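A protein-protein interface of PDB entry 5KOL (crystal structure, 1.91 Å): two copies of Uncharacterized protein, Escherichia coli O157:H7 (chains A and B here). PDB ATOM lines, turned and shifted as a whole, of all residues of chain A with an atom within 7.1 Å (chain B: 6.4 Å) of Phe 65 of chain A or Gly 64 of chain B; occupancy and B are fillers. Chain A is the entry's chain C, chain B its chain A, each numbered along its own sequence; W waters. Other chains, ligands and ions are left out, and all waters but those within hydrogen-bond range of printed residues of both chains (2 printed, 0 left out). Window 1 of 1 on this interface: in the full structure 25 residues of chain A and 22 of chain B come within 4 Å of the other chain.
The backbone carbonyl oxygen (O) of Gly 62 of chain B sits at hydrogen-bond distance from the backbone NH (N) of Phe 68 of chain A, at 2.8 Å.
O of Val 66 of chain A lies within hydrogen-bond range of N of Gly 64 of chain B.
The backbone NH (N) of Val 66 of chain B lies within hydrogen-bond range of the backbone carbonyl oxygen (O) of Gly 64 of chain A (2.9 Å).
The backbone carbonyl oxygen (O) of Val 66 of chain A sits close to the backbone carbonyl oxygen (O) of Gly 62 of chain B (3.2 Å).
The backbone carbonyl oxygen (O) of Ala 63 of chain B lies within hydrogen-bond range of the side-chain hydroxyl (OG1) of Thr 37 of chain B (2.8 Å).
The backbone NH (N) of Phe 65 of chain B is in hydrogen-bond range of the backbone carbonyl oxygen (O) of Thr 38 of chain B (2.9 Å).
The backbone carbonyl oxygen (O) of Ile 76 of chain B lies within hydrogen-bond range of the guanidinium group (NE) of Arg 105 of chain B (2.8 Å).
O of Thr 38 of chain A lies within hydrogen-bond range of N of Phe 65 of chain A (2.8 Å).
O of Glu 40 of chain A sits at hydrogen-bond distance from N of Thr 67 of chain A, at 2.9 Å.
The side-chain hydroxyl (OG) of Ser 41 of chain A lies within hydrogen-bond range of the backbone carbonyl oxygen (O) of Thr 67 of chain A (3.2 Å).
Gly 44 of chain A touches Ala 48 of chain B.
Ala 63 of chain A touches Val 66 of chain B (CA to O, 3.4 Å).
Phe 65 of chain B touches Gly 64 of chain A (C to O, 3.8 Å).
Phe 65 of chain A touches Gly 64 of chain B (CA to O, 3.7 Å).
CZ of Phe 65 of chain A touches CD1 of Ile 76 of chain B, 3.8 Å away.
Ala 63 of chain B touches Val 66 of chain A (CA to O, 3.4 Å).
Thr 67 of chain A touches Gly 62 of chain B.
Gly 62 of chain B touches Ala 72 of chain A.
Phe 65 of chain B touches Ile 76 of chain A.
Ile 76 of chain A touches Arg 105 of chain B (CD1 to O, 3.4 Å).
Phe 65 of chain A touches just these residues of chain B: Gly 64 (3.7 Å) and Ile 76 (3.8 Å).
Of the printed residues of chain B, Ile 76 of chain A touches Phe 65 (3.6 Å) and Arg 105 (3.4 Å).
Of the printed residues of chain A, Gly 62 of chain B touches Val 66 (3.2 Å), Thr 67 (3.4 Å), Phe 68 (2.8 Å) and Ala 72 (3.4 Å).
Of the printed residues of chain A, Gly 64 of chain B touches Phe 65 (3.7 Å) and Val 66 (2.9 Å).
Of the printed residues of chain A, Arg 105 of chain B touches Ile 76 (3.4 Å) and Arg 105 (3.6 Å).
The nearest residue of chain B that does not touch Phe 65 of chain A is Phe 65 of chain B (4.02 Å).
The nearest residue of chain A that does not touch Gly 64 of chain B is Gly 64 of chain A (4.04 Å).
Hydrophobic or aromatic side chains of chain B that line the printed part of chain A: Ala 48, Phe 65, Val 66 and Ile 76.
Along chain B the printed residues that touch a printed residue of chain A span positions 48 to 105.
Printed residues of chain A that touch a printed residue of chain B: Gly 44, Ala 63, Gly 64, Phe 65, Val 66, Thr 67, Phe 68, Ala 72, Ile 76 and Arg 105.
Hydrophobic or aromatic side chains of chain A within 4 Å of the printed part of chain B: Phe 65, Val 66, Phe 68, Ala 72 and Ile 76.
Along chain A the printed residues that touch a printed residue of chain B span positions 44 to 105.
Among the printed residues, no Asp or Glu carboxylate lies within 4 Å of a Lys or Arg side-chain nitrogen of the other chain.
Ala 63 of chain A touches Val 66 of chain B, and with the chains exchanged Val 66 of chain A touches Ala 63 of chain B.
Gly 64 of chain A touches Phe 65 of chain B, and with the chains exchanged Phe 65 of chain A touches Gly 64 of chain B.
Gly 64 of chain A touches Val 66 of chain B, and with the chains exchanged Val 66 of chain A touches Gly 64 of chain B.
Ile 76 of chain A touches Arg 105 of chain B, and with the chains exchanged Arg 105 of chain A touches Ile 76 of chain B.
Positions printed for both chains: 37, 38, 39, 40, 48, 61, 63, 64, 65, 66, 76 and 105.
Water W2 lies within hydrogen-bond range of NH1 of Arg 105 of chain B, NE of Arg 105 of chain A and O of Ile 76 of chain A.
Water W1 lies within hydrogen-bond range of the backbone carbonyl oxygen (O) of Val 66 of chain B (2.8 Å) and the backbone carbonyl oxygen (O) of Gly 64 of chain A (3.0 Å).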
ATOM      1  N   THR A  37      21.483  11.480  13.791  1.00  0.00           N
ATOM      2  CA  THR A  37      20.412  10.499  13.915  1.00  0.00           C
ATOM      3  C   THR A  37      20.506   9.890  15.309  1.00  0.00           C
ATOM      4  O   THR A  37      21.554   9.933  15.944  1.00  0.00           O
ATOM      5  CB  THR A  37      20.495   9.405  12.827  1.00  0.00           C
ATOM      6  OG1 THR A  37      19.374   8.518  12.939  1.00  0.00           O
ATOM      7  CG2 THR A  37      21.781   8.591  12.968  1.00  0.00           C
ATOM      8  N   THR A  38      19.396   9.337  15.801  1.00  0.00           N
ATOM      9  CA  THR A  38      19.363   8.814  17.160  1.00  0.00           C
ATOM     10  C   THR A  38      18.698   7.448  17.209  1.00  0.00           C
ATOM     11  O   THR A  38      17.861   7.111  16.367  1.00  0.00           O
ATOM     12  CB  THR A  38      18.631   9.779  18.115  1.00  0.00           C
ATOM     13  OG1 THR A  38      17.285   9.972  17.648  1.00  0.00           O
ATOM     14  CG2 THR A  38      19.361  11.100  18.219  1.00  0.00           C
ATOM     15  N   ALA A  39      19.086   6.669  18.219  1.00  0.00           N
ATOM     16  CA  ALA A  39      18.552   5.332  18.461  1.00  0.00           C
ATOM     17  C   ALA A  39      18.308   5.221  19.952  1.00  0.00           C
ATOM     18  O   ALA A  39      19.231   5.446  20.735  1.00  0.00           O
ATOM     19  CB  ALA A  39      19.539   4.249  18.002  1.00  0.00           C
ATOM     20  N   GLU A  40      17.085   4.894  20.358  1.00  0.00           N
ATOM     21  CA  GLU A  40      16.826   4.841  21.786  1.00  0.00           C
ATOM     22  C   GLU A  40      15.920   3.671  22.118  1.00  0.00           C
ATOM     23  O   GLU A  40      15.206   3.129  21.268  1.00  0.00           O
ATOM     24  CB  GLU A  40      16.237   6.156  22.316  1.00  0.00           C
ATOM     25  CG  GLU A  40      15.061   6.694  21.596  1.00  0.00           C
ATOM     26  CD  GLU A  40      14.722   8.118  22.029  1.00  0.00           C
ATOM     27  OE1 GLU A  40      14.538   8.369  23.249  1.00  0.00           O
ATOM     28  OE2 GLU A  40      14.635   8.996  21.143  1.00  0.00           O
ATOM     29  N   SER A  41      15.960   3.292  23.390  1.00  0.00           N
ATOM     30  CA  SER A  41      15.152   2.180  23.854  1.00  0.00           C
ATOM     31  C   SER A  41      14.338   2.618  25.066  1.00  0.00           C
ATOM     32  O   SER A  41      13.169   2.999  24.930  1.00  0.00           O
ATOM     33  CB  SER A  41      16.056   0.987  24.165  1.00  0.00           C
ATOM     34  OG  SER A  41      15.298  -0.164  24.474  1.00  0.00           O
ATOM     35  N   GLY A  44      12.435   5.820  25.059  1.00  0.00           N
ATOM     36  CA  GLY A  44      11.107   5.709  24.471  1.00  0.00           C
ATOM     37  C   GLY A  44      10.772   6.684  23.364  1.00  0.00           C
ATOM     38  O   GLY A  44       9.631   6.688  22.898  1.00  0.00           O
ATOM     39  N   GLY A  45      11.724   7.493  22.903  1.00  0.00           N
ATOM     40  CA  GLY A  45      11.431   8.544  21.941  1.00  0.00           C
ATOM     41  C   GLY A  45      11.519   9.943  22.508  1.00  0.00           C
ATOM     42  O   GLY A  45      11.321  10.909  21.758  1.00  0.00           O
ATOM     43  N   ALA A  48      14.459  11.806  20.734  1.00  0.00           N
ATOM     44  CA  ALA A  48      14.043  12.349  19.444  1.00  0.00           C
ATOM     45  C   ALA A  48      13.109  13.544  19.621  1.00  0.00           C
ATOM     46  O   ALA A  48      13.246  14.554  18.920  1.00  0.00           O
ATOM     47  CB  ALA A  48      13.396  11.254  18.594  1.00  0.00           C
ATOM     48  N   TYR A  61      18.697  17.339  11.669  1.00  0.00           N
ATOM     49  CA  TYR A  61      18.140  16.113  12.230  1.00  0.00           C
ATOM     50  C   TYR A  61      16.948  15.659  11.406  1.00  0.00           C
ATOM     51  O   TYR A  61      16.081  16.469  11.069  1.00  0.00           O
ATOM     52  CB  TYR A  61      17.718  16.320  13.690  1.00  0.00           C
ATOM     53  CG  TYR A  61      17.144  15.097  14.379  1.00  0.00           C
ATOM     54  CD1 TYR A  61      17.957  14.033  14.746  1.00  0.00           C
ATOM     55  CD2 TYR A  61      15.792  15.025  14.697  1.00  0.00           C
ATOM     56  CE1 TYR A  61      17.447  12.926  15.396  1.00  0.00           C
ATOM     57  CE2 TYR A  61      15.268  13.922  15.355  1.00  0.00           C
ATOM     58  CZ  TYR A  61      16.096  12.876  15.705  1.00  0.00           C
ATOM     59  OH  TYR A  61      15.574  11.781  16.358  1.00  0.00           O
ATOM     60  N   ALA A  63      16.094  11.617  11.297  1.00  0.00           N
ATOM     61  CA  ALA A  63      15.670  10.242  11.541  1.00  0.00           C
ATOM     62  C   ALA A  63      15.990   9.821  12.966  1.00  0.00           C
ATOM     63  O   ALA A  63      17.158   9.830  13.376  1.00  0.00           O
ATOM     64  CB  ALA A  63      16.334   9.297  10.529  1.00  0.00           C
ATOM     65  N   GLY A  64      14.957   9.467  13.724  1.00  0.00           N
ATOM     66  CA  GLY A  64      15.122   8.888  15.051  1.00  0.00           C
ATOM     67  C   GLY A  64      14.473   7.526  15.098  1.00  0.00           C
ATOM     68  O   GLY A  64      13.408   7.313  14.511  1.00  0.00           O
ATOM     69  N   PHE A  65      15.130   6.585  15.779  1.00  0.00           N
ATOM     70  CA  PHE A  65      14.646   5.221  15.918  1.00  0.00           C
ATOM     71  C   PHE A  65      14.340   4.911  17.379  1.00  0.00           C
ATOM     72  O   PHE A  65      15.143   5.214  18.266  1.00  0.00           O
ATOM     73  CB  PHE A  65      15.680   4.238  15.368  1.00  0.00           C
ATOM     74  CG  PHE A  65      16.061   4.523  13.931  1.00  0.00           C
ATOM     75  CD1 PHE A  65      15.252   4.071  12.893  1.00  0.00           C
ATOM     76  CD2 PHE A  65      17.211   5.251  13.626  1.00  0.00           C
ATOM     77  CE1 PHE A  65      15.596   4.335  11.567  1.00  0.00           C
ATOM     78  CE2 PHE A  65      17.562   5.522  12.307  1.00  0.00           C
ATOM     79  CZ  PHE A  65      16.747   5.061  11.277  1.00  0.00           C
ATOM     80  N   VAL A  66      13.180   4.315  17.627  1.00  0.00           N
ATOM     81  CA  VAL A  66      12.893   3.699  18.919  1.00  0.00           C
ATOM     82  C   VAL A  66      12.836   2.192  18.686  1.00  0.00           C
ATOM     83  O   VAL A  66      12.033   1.708  17.878  1.00  0.00           O
ATOM     84  CB  VAL A  66      11.594   4.237  19.539  1.00  0.00           C
ATOM     85  CG1 VAL A  66      11.385   3.634  20.921  1.00  0.00           C
ATOM     86  CG2 VAL A  66      11.638   5.765  19.643  1.00  0.00           C
ATOM     87  N   THR A  67      13.710   1.455  19.365  1.00  0.00           N
ATOM     88  CA  THR A  67      13.787   0.000  19.249  1.00  0.00           C
ATOM     89  C   THR A  67      13.691  -0.554  20.668  1.00  0.00           C
ATOM     90  O   THR A  67      14.704  -0.741  21.347  1.00  0.00           O
ATOM     91  CB  THR A  67      15.081  -0.437  18.535  1.00  0.00           C
ATOM     92  OG1 THR A  67      16.210   0.088  19.233  1.00  0.00           O
ATOM     93  CG2 THR A  67      15.100   0.073  17.076  1.00  0.00           C
ATOM     94  N   PHE A  68      12.462  -0.829  21.110  1.00  0.00           N
ATOM     95  CA  PHE A  68      12.227  -1.158  22.511  1.00  0.00           C
ATOM     96  C   PHE A  68      12.492  -2.628  22.822  1.00  0.00           C
ATOM     97  O   PHE A  68      12.674  -2.971  23.996  1.00  0.00           O
ATOM     98  CB  PHE A  68      10.784  -0.769  22.880  1.00  0.00           C
ATOM     99  CG  PHE A  68      10.541  -0.567  24.367  1.00  0.00           C
ATOM    100  CD1 PHE A  68      10.920   0.613  24.999  1.00  0.00           C
ATOM    101  CD2 PHE A  68       9.915  -1.548  25.122  1.00  0.00           C
ATOM    102  CE1 PHE A  68      10.689   0.806  26.364  1.00  0.00           C
ATOM    103  CE2 PHE A  68       9.681  -1.366  26.489  1.00  0.00           C
ATOM    104  CZ  PHE A  68      10.066  -0.188  27.107  1.00  0.00           C
ATOM    105  N   ALA A  72      13.223  -5.571  17.608  1.00  0.00           N
ATOM    106  CA  ALA A  72      13.357  -4.275  16.950  1.00  0.00           C
ATOM    107  C   ALA A  72      14.821  -3.899  16.767  1.00  0.00           C
ATOM    108  O   ALA A  72      15.220  -3.433  15.693  1.00  0.00           O
ATOM    109  CB  ALA A  72      12.622  -3.200  17.748  1.00  0.00           C
ATOM    110  N   ILE A  76      15.694  -3.407  12.947  1.00  0.00           N
ATOM    111  CA  ILE A  76      15.821  -2.021  12.498  1.00  0.00           C
ATOM    112  C   ILE A  76      17.283  -1.587  12.435  1.00  0.00           C
ATOM    113  O   ILE A  76      17.693  -0.895  11.499  1.00  0.00           O
ATOM    114  CB  ILE A  76      14.999  -1.095  13.410  1.00  0.00           C
ATOM    115  CG1 ILE A  76      13.538  -1.545  13.438  1.00  0.00           C
ATOM    116  CG2 ILE A  76      15.125   0.361  12.964  1.00  0.00           C
ATOM    117  CD1 ILE A  76      12.918  -1.647  12.059  1.00  0.00           C
ATOM    118  N   LEU A  77      18.095  -1.971  13.418  1.00  0.00           N
ATOM    119  CA  LEU A  77      19.442  -1.415  13.550  1.00  0.00           C
ATOM    120  C   LEU A  77      20.533  -2.466  13.390  1.00  0.00           C
ATOM    121  O   LEU A  77      21.712  -2.163  13.625  1.00  0.00           O
ATOM    122  CB  LEU A  77      19.590  -0.711  14.901  1.00  0.00           C
ATOM    123  CG  LEU A  77      18.629   0.445  15.166  1.00  0.00           C
ATOM    124  CD1 LEU A  77      18.784   0.930  16.614  1.00  0.00           C
ATOM    125  CD2 LEU A  77      18.912   1.582  14.194  1.00  0.00           C
ATOM    126  N   MET A  98      23.811  -0.115  18.083  1.00  0.00           N
ATOM    127  CA  MET A  98      22.688   0.771  17.790  1.00  0.00           C
ATOM    128  C   MET A  98      23.159   2.088  17.188  1.00  0.00           C
ATOM    129  O   MET A  98      22.513   2.614  16.273  1.00  0.00           O
ATOM    130  CB  MET A  98      21.808   1.043  19.023  1.00  0.00           C
ATOM    131  CG  MET A  98      21.089  -0.151  19.614  1.00  0.00           C
ATOM    132  SD  MET A  98      20.498   0.178  21.301  1.00  0.00           S
ATOM    133  CE  MET A  98      19.197   1.373  21.009  1.00  0.00           C
ATOM    134  N   GLY A 101      24.396   1.276  13.626  1.00  0.00           N
ATOM    135  CA  GLY A 101      23.251   0.875  12.825  1.00  0.00           C
ATOM    136  C   GLY A 101      22.368   2.042  12.424  1.00  0.00           C
ATOM    137  O   GLY A 101      21.803   2.053  11.327  1.00  0.00           O
ATOM    138  N   ALA A 102      22.226   3.032  13.312  1.00  0.00           N
ATOM    139  CA  ALA A 102      21.439   4.214  12.979  1.00  0.00           C
ATOM    140  C   ALA A 102      22.129   5.040  11.905  1.00  0.00           C
ATOM    141  O   ALA A 102      21.478   5.522  10.975  1.00  0.00           O
ATOM    142  CB  ALA A 102      21.201   5.062  14.229  1.00  0.00           C
ATOM    143  N   ILE A 103      23.446   5.225  12.027  1.00  0.00           N
ATOM    144  CA  ILE A 103      24.216   5.901  10.976  1.00  0.00           C
ATOM    145  C   ILE A 103      23.910   5.292   9.611  1.00  0.00           C
ATOM    146  O   ILE A 103      23.643   6.009   8.640  1.00  0.00           O
ATOM    147  CB  ILE A 103      25.721   5.855  11.294  1.00  0.00           C
ATOM    148  CG1 ILE A 103      26.052   6.752  12.494  1.00  0.00           C
ATOM    149  CG2 ILE A 103      26.559   6.254  10.061  1.00  0.00           C
ATOM    150  CD1 ILE A 103      26.055   8.237  12.190  1.00  0.00           C
ATOM    151  N   GLU A 104      23.906   3.958   9.526  1.00  0.00           N
ATOM    152  CA  GLU A 104      23.722   3.302   8.231  1.00  0.00           C
ATOM    153  C   GLU A 104      22.311   3.518   7.690  1.00  0.00           C
ATOM    154  O   GLU A 104      22.139   3.858   6.514  1.00  0.00           O
ATOM    155  CB  GLU A 104      24.026   1.806   8.337  1.00  0.00           C
ATOM    156  CG  GLU A 104      25.241   1.440   9.187  1.00  0.00           C
ATOM    157  CD  GLU A 104      26.525   2.157   8.769  1.00  0.00           C
ATOM    158  OE1 GLU A 104      27.329   2.512   9.664  1.00  0.00           O
ATOM    159  OE2 GLU A 104      26.735   2.361   7.551  1.00  0.00           O
ATOM    160  N   ARG A 105      21.287   3.322   8.531  1.00  0.00           N
ATOM    161  CA  ARG A 105      19.909   3.435   8.060  1.00  0.00           C
ATOM    162  C   ARG A 105      19.568   4.857   7.635  1.00  0.00           C
ATOM    163  O   ARG A 105      18.775   5.058   6.709  1.00  0.00           O
ATOM    164  CB  ARG A 105      18.922   2.977   9.141  1.00  0.00           C
ATOM    165  CG  ARG A 105      18.954   1.502   9.458  1.00  0.00           C
ATOM    166  CD  ARG A 105      19.010   0.665   8.188  1.00  0.00           C
ATOM    167  NE  ARG A 105      18.721  -0.742   8.452  1.00  0.00           N
ATOM    168  CZ  ARG A 105      19.587  -1.596   8.991  1.00  0.00           C
ATOM    169  NH1 ARG A 105      20.804  -1.189   9.336  1.00  0.00           N
ATOM    170  NH2 ARG A 105      19.233  -2.859   9.200  1.00  0.00           N
ATOM    171  N   ALA A 106      20.111   5.853   8.331  1.00  0.00           N
ATOM    172  CA  ALA A 106      19.797   7.248   8.046  1.00  0.00           C
ATOM    173  C   ALA A 106      20.740   7.895   7.035  1.00  0.00           C
ATOM    174  O   ALA A 106      20.411   8.964   6.515  1.00  0.00           O
ATOM    175  CB  ALA A 106      19.819   8.068   9.345  1.00  0.00           C
ATOM    176  N   ILE A 112      23.626   9.220  18.344  1.00  0.00           N
ATOM    177  CA  ILE A 112      23.547   8.934  19.774  1.00  0.00           C
ATOM    178  C   ILE A 112      22.721   7.665  19.945  1.00  0.00           C
ATOM    179  O   ILE A 112      21.667   7.530  19.312  1.00  0.00           O
ATOM    180  CB  ILE A 112      22.852  10.079  20.539  1.00  0.00           C
ATOM    181  CG1 ILE A 112      23.332  11.445  20.067  1.00  0.00           C
ATOM    182  CG2 ILE A 112      22.958   9.874  22.046  1.00  0.00           C
ATOM    183  CD1 ILE A 112      22.659  12.603  20.789  1.00  0.00           C
ATOM    184  N   THR B  37       3.453  -0.897  15.151  1.00  0.00           N
ATOM    185  CA  THR B  37       4.569  -0.013  14.857  1.00  0.00           C
ATOM    186  C   THR B  37       4.001   1.375  14.579  1.00  0.00           C
ATOM    187  O   THR B  37       2.818   1.524  14.268  1.00  0.00           O
ATOM    188  CB  THR B  37       5.397  -0.523  13.662  1.00  0.00           C
ATOM    189  OG1 THR B  37       6.549   0.323  13.461  1.00  0.00           O
ATOM    190  CG2 THR B  37       4.532  -0.556  12.393  1.00  0.00           C
ATOM    191  N   THR B  38       4.847   2.393  14.714  1.00  0.00           N
ATOM    192  CA  THR B  38       4.415   3.786  14.595  1.00  0.00           C
ATOM    193  C   THR B  38       5.399   4.574  13.744  1.00  0.00           C
ATOM    194  O   THR B  38       6.591   4.260  13.694  1.00  0.00           O
ATOM    195  CB  THR B  38       4.294   4.471  15.966  1.00  0.00           C
ATOM    196  OG1 THR B  38       5.577   4.456  16.622  1.00  0.00           O
ATOM    197  CG2 THR B  38       3.276   3.726  16.823  1.00  0.00           C
ATOM    198  N   ALA B  39       4.881   5.610  13.086  1.00  0.00           N
ATOM    199  CA  ALA B  39       5.664   6.531  12.278  1.00  0.00           C
ATOM    200  C   ALA B  39       5.149   7.930  12.572  1.00  0.00           C
ATOM    201  O   ALA B  39       3.945   8.169  12.482  1.00  0.00           O
ATOM    202  CB  ALA B  39       5.535   6.210  10.771  1.00  0.00           C
ATOM    203  N   GLU B  40       6.032   8.860  12.928  1.00  0.00           N
ATOM    204  CA  GLU B  40       5.528  10.190  13.245  1.00  0.00           C
ATOM    205  C   GLU B  40       6.492  11.255  12.765  1.00  0.00           C
ATOM    206  O   GLU B  40       7.684  11.007  12.579  1.00  0.00           O
ATOM    207  CB  GLU B  40       5.250  10.359  14.751  1.00  0.00           C
ATOM    208  CG  GLU B  40       6.377   9.907  15.622  1.00  0.00           C
ATOM    209  CD  GLU B  40       5.996   9.818  17.089  1.00  0.00           C
ATOM    210  OE1 GLU B  40       5.390  10.778  17.615  1.00  0.00           O
ATOM    211  OE2 GLU B  40       6.360   8.806  17.719  1.00  0.00           O
ATOM    212  N   ALA B  48       5.447   7.357  20.215  1.00  0.00           N
ATOM    213  CA  ALA B  48       6.289   6.253  20.670  1.00  0.00           C
ATOM    214  C   ALA B  48       6.480   6.283  22.179  1.00  0.00           C
ATOM    215  O   ALA B  48       6.391   5.238  22.837  1.00  0.00           O
ATOM    216  CB  ALA B  48       7.642   6.304  19.963  1.00  0.00           C
ATOM    217  N   TYR B  61       4.720  -3.998  21.104  1.00  0.00           N
ATOM    218  CA  TYR B  61       5.316  -2.840  20.434  1.00  0.00           C
ATOM    219  C   TYR B  61       6.830  -2.853  20.564  1.00  0.00           C
ATOM    220  O   TYR B  61       7.355  -2.930  21.676  1.00  0.00           O
ATOM    221  CB  TYR B  61       4.770  -1.530  21.019  1.00  0.00           C
ATOM    222  CG  TYR B  61       5.331  -0.247  20.406  1.00  0.00           C
ATOM    223  CD1 TYR B  61       4.961   0.156  19.126  1.00  0.00           C
ATOM    224  CD2 TYR B  61       6.187   0.583  21.136  1.00  0.00           C
ATOM    225  CE1 TYR B  61       5.456   1.351  18.570  1.00  0.00           C
ATOM    226  CE2 TYR B  61       6.690   1.771  20.596  1.00  0.00           C
ATOM    227  CZ  TYR B  61       6.312   2.147  19.313  1.00  0.00           C
ATOM    228  OH  TYR B  61       6.785   3.322  18.785  1.00  0.00           O
ATOM    229  N   GLY B  62       7.529  -2.722  19.435  1.00  0.00           N
ATOM    230  CA  GLY B  62       8.972  -2.607  19.490  1.00  0.00           C
ATOM    231  C   GLY B  62       9.563  -1.467  18.683  1.00  0.00           C
ATOM    232  O   GLY B  62      10.533  -0.846  19.121  1.00  0.00           O
ATOM    233  N   ALA B  63       8.984  -1.165  17.522  1.00  0.00           N
ATOM    234  CA  ALA B  63       9.619  -0.313  16.521  1.00  0.00           C
ATOM    235  C   ALA B  63       8.845   0.981  16.343  1.00  0.00           C
ATOM    236  O   ALA B  63       7.679   0.965  15.918  1.00  0.00           O
ATOM    237  CB  ALA B  63       9.730  -1.049  15.180  1.00  0.00           C
ATOM    238  N   GLY B  64       9.494   2.104  16.602  1.00  0.00           N
ATOM    239  CA  GLY B  64       8.924   3.412  16.344  1.00  0.00           C
ATOM    240  C   GLY B  64       9.851   4.227  15.473  1.00  0.00           C
ATOM    241  O   GLY B  64      11.065   4.232  15.681  1.00  0.00           O
ATOM    242  N   PHE B  65       9.278   4.930  14.500  1.00  0.00           N
ATOM    243  CA  PHE B  65      10.056   5.738  13.575  1.00  0.00           C
ATOM    244  C   PHE B  65       9.679   7.198  13.753  1.00  0.00           C
ATOM    245  O   PHE B  65       8.492   7.522  13.872  1.00  0.00           O
ATOM    246  CB  PHE B  65       9.809   5.279  12.133  1.00  0.00           C
ATOM    247  CG  PHE B  65      10.125   3.828  11.917  1.00  0.00           C
ATOM    248  CD1 PHE B  65      11.444   3.420  11.765  1.00  0.00           C
ATOM    249  CD2 PHE B  65       9.121   2.875  11.893  1.00  0.00           C
ATOM    250  CE1 PHE B  65      11.753   2.087  11.583  1.00  0.00           C
ATOM    251  CE2 PHE B  65       9.426   1.530  11.700  1.00  0.00           C
ATOM    252  CZ  PHE B  65      10.747   1.143  11.548  1.00  0.00           C
ATOM    253  N   VAL B  66      10.688   8.058  13.815  1.00  0.00           N
ATOM    254  CA  VAL B  66      10.507   9.496  13.770  1.00  0.00           C
ATOM    255  C   VAL B  66      11.185   9.982  12.503  1.00  0.00           C
ATOM    256  O   VAL B  66      12.394   9.784  12.326  1.00  0.00           O
ATOM    257  CB  VAL B  66      11.078  10.190  15.019  1.00  0.00           C
ATOM    258  CG1 VAL B  66      10.921  11.674  14.901  1.00  0.00           C
ATOM    259  CG2 VAL B  66      10.351   9.680  16.290  1.00  0.00           C
ATOM    260  N   ILE B  76      13.582   6.223   5.174  1.00  0.00           N
ATOM    261  CA  ILE B  76      13.203   5.251   6.195  1.00  0.00           C
ATOM    262  C   ILE B  76      11.861   4.593   5.867  1.00  0.00           C
ATOM    263  O   ILE B  76      11.670   3.392   6.099  1.00  0.00           O
ATOM    264  CB  ILE B  76      13.165   5.940   7.580  1.00  0.00           C
ATOM    265  CG1 ILE B  76      14.498   6.633   7.882  1.00  0.00           C
ATOM    266  CG2 ILE B  76      12.786   4.941   8.680  1.00  0.00           C
ATOM    267  CD1 ILE B  76      15.715   5.775   7.638  1.00  0.00           C
ATOM    268  N   ARG B 105       9.147  -1.901   7.246  1.00  0.00           N
ATOM    269  CA  ARG B 105      10.425  -1.853   7.951  1.00  0.00           C
ATOM    270  C   ARG B 105      10.399  -2.693   9.224  1.00  0.00           C
ATOM    271  O   ARG B 105      11.397  -3.330   9.573  1.00  0.00           O
ATOM    272  CB  ARG B 105      10.775  -0.401   8.284  1.00  0.00           C
ATOM    273  CG  ARG B 105      11.387   0.392   7.149  1.00  0.00           C
ATOM    274  CD  ARG B 105      12.900   0.267   7.162  1.00  0.00           C
ATOM    275  NE  ARG B 105      13.549   1.277   6.332  1.00  0.00           N
ATOM    276  CZ  ARG B 105      14.866   1.416   6.227  1.00  0.00           C
ATOM    277  NH1 ARG B 105      15.670   0.612   6.908  1.00  0.00           N
ATOM    278  NH2 ARG B 105      15.381   2.357   5.444  1.00  0.00           N
HETATM  279  O   HOH W   1      13.076   7.171  11.545  1.00  0.00           O
HETATM  280  O   HOH W   2      16.123  -0.369   9.183  1.00  0.00           O
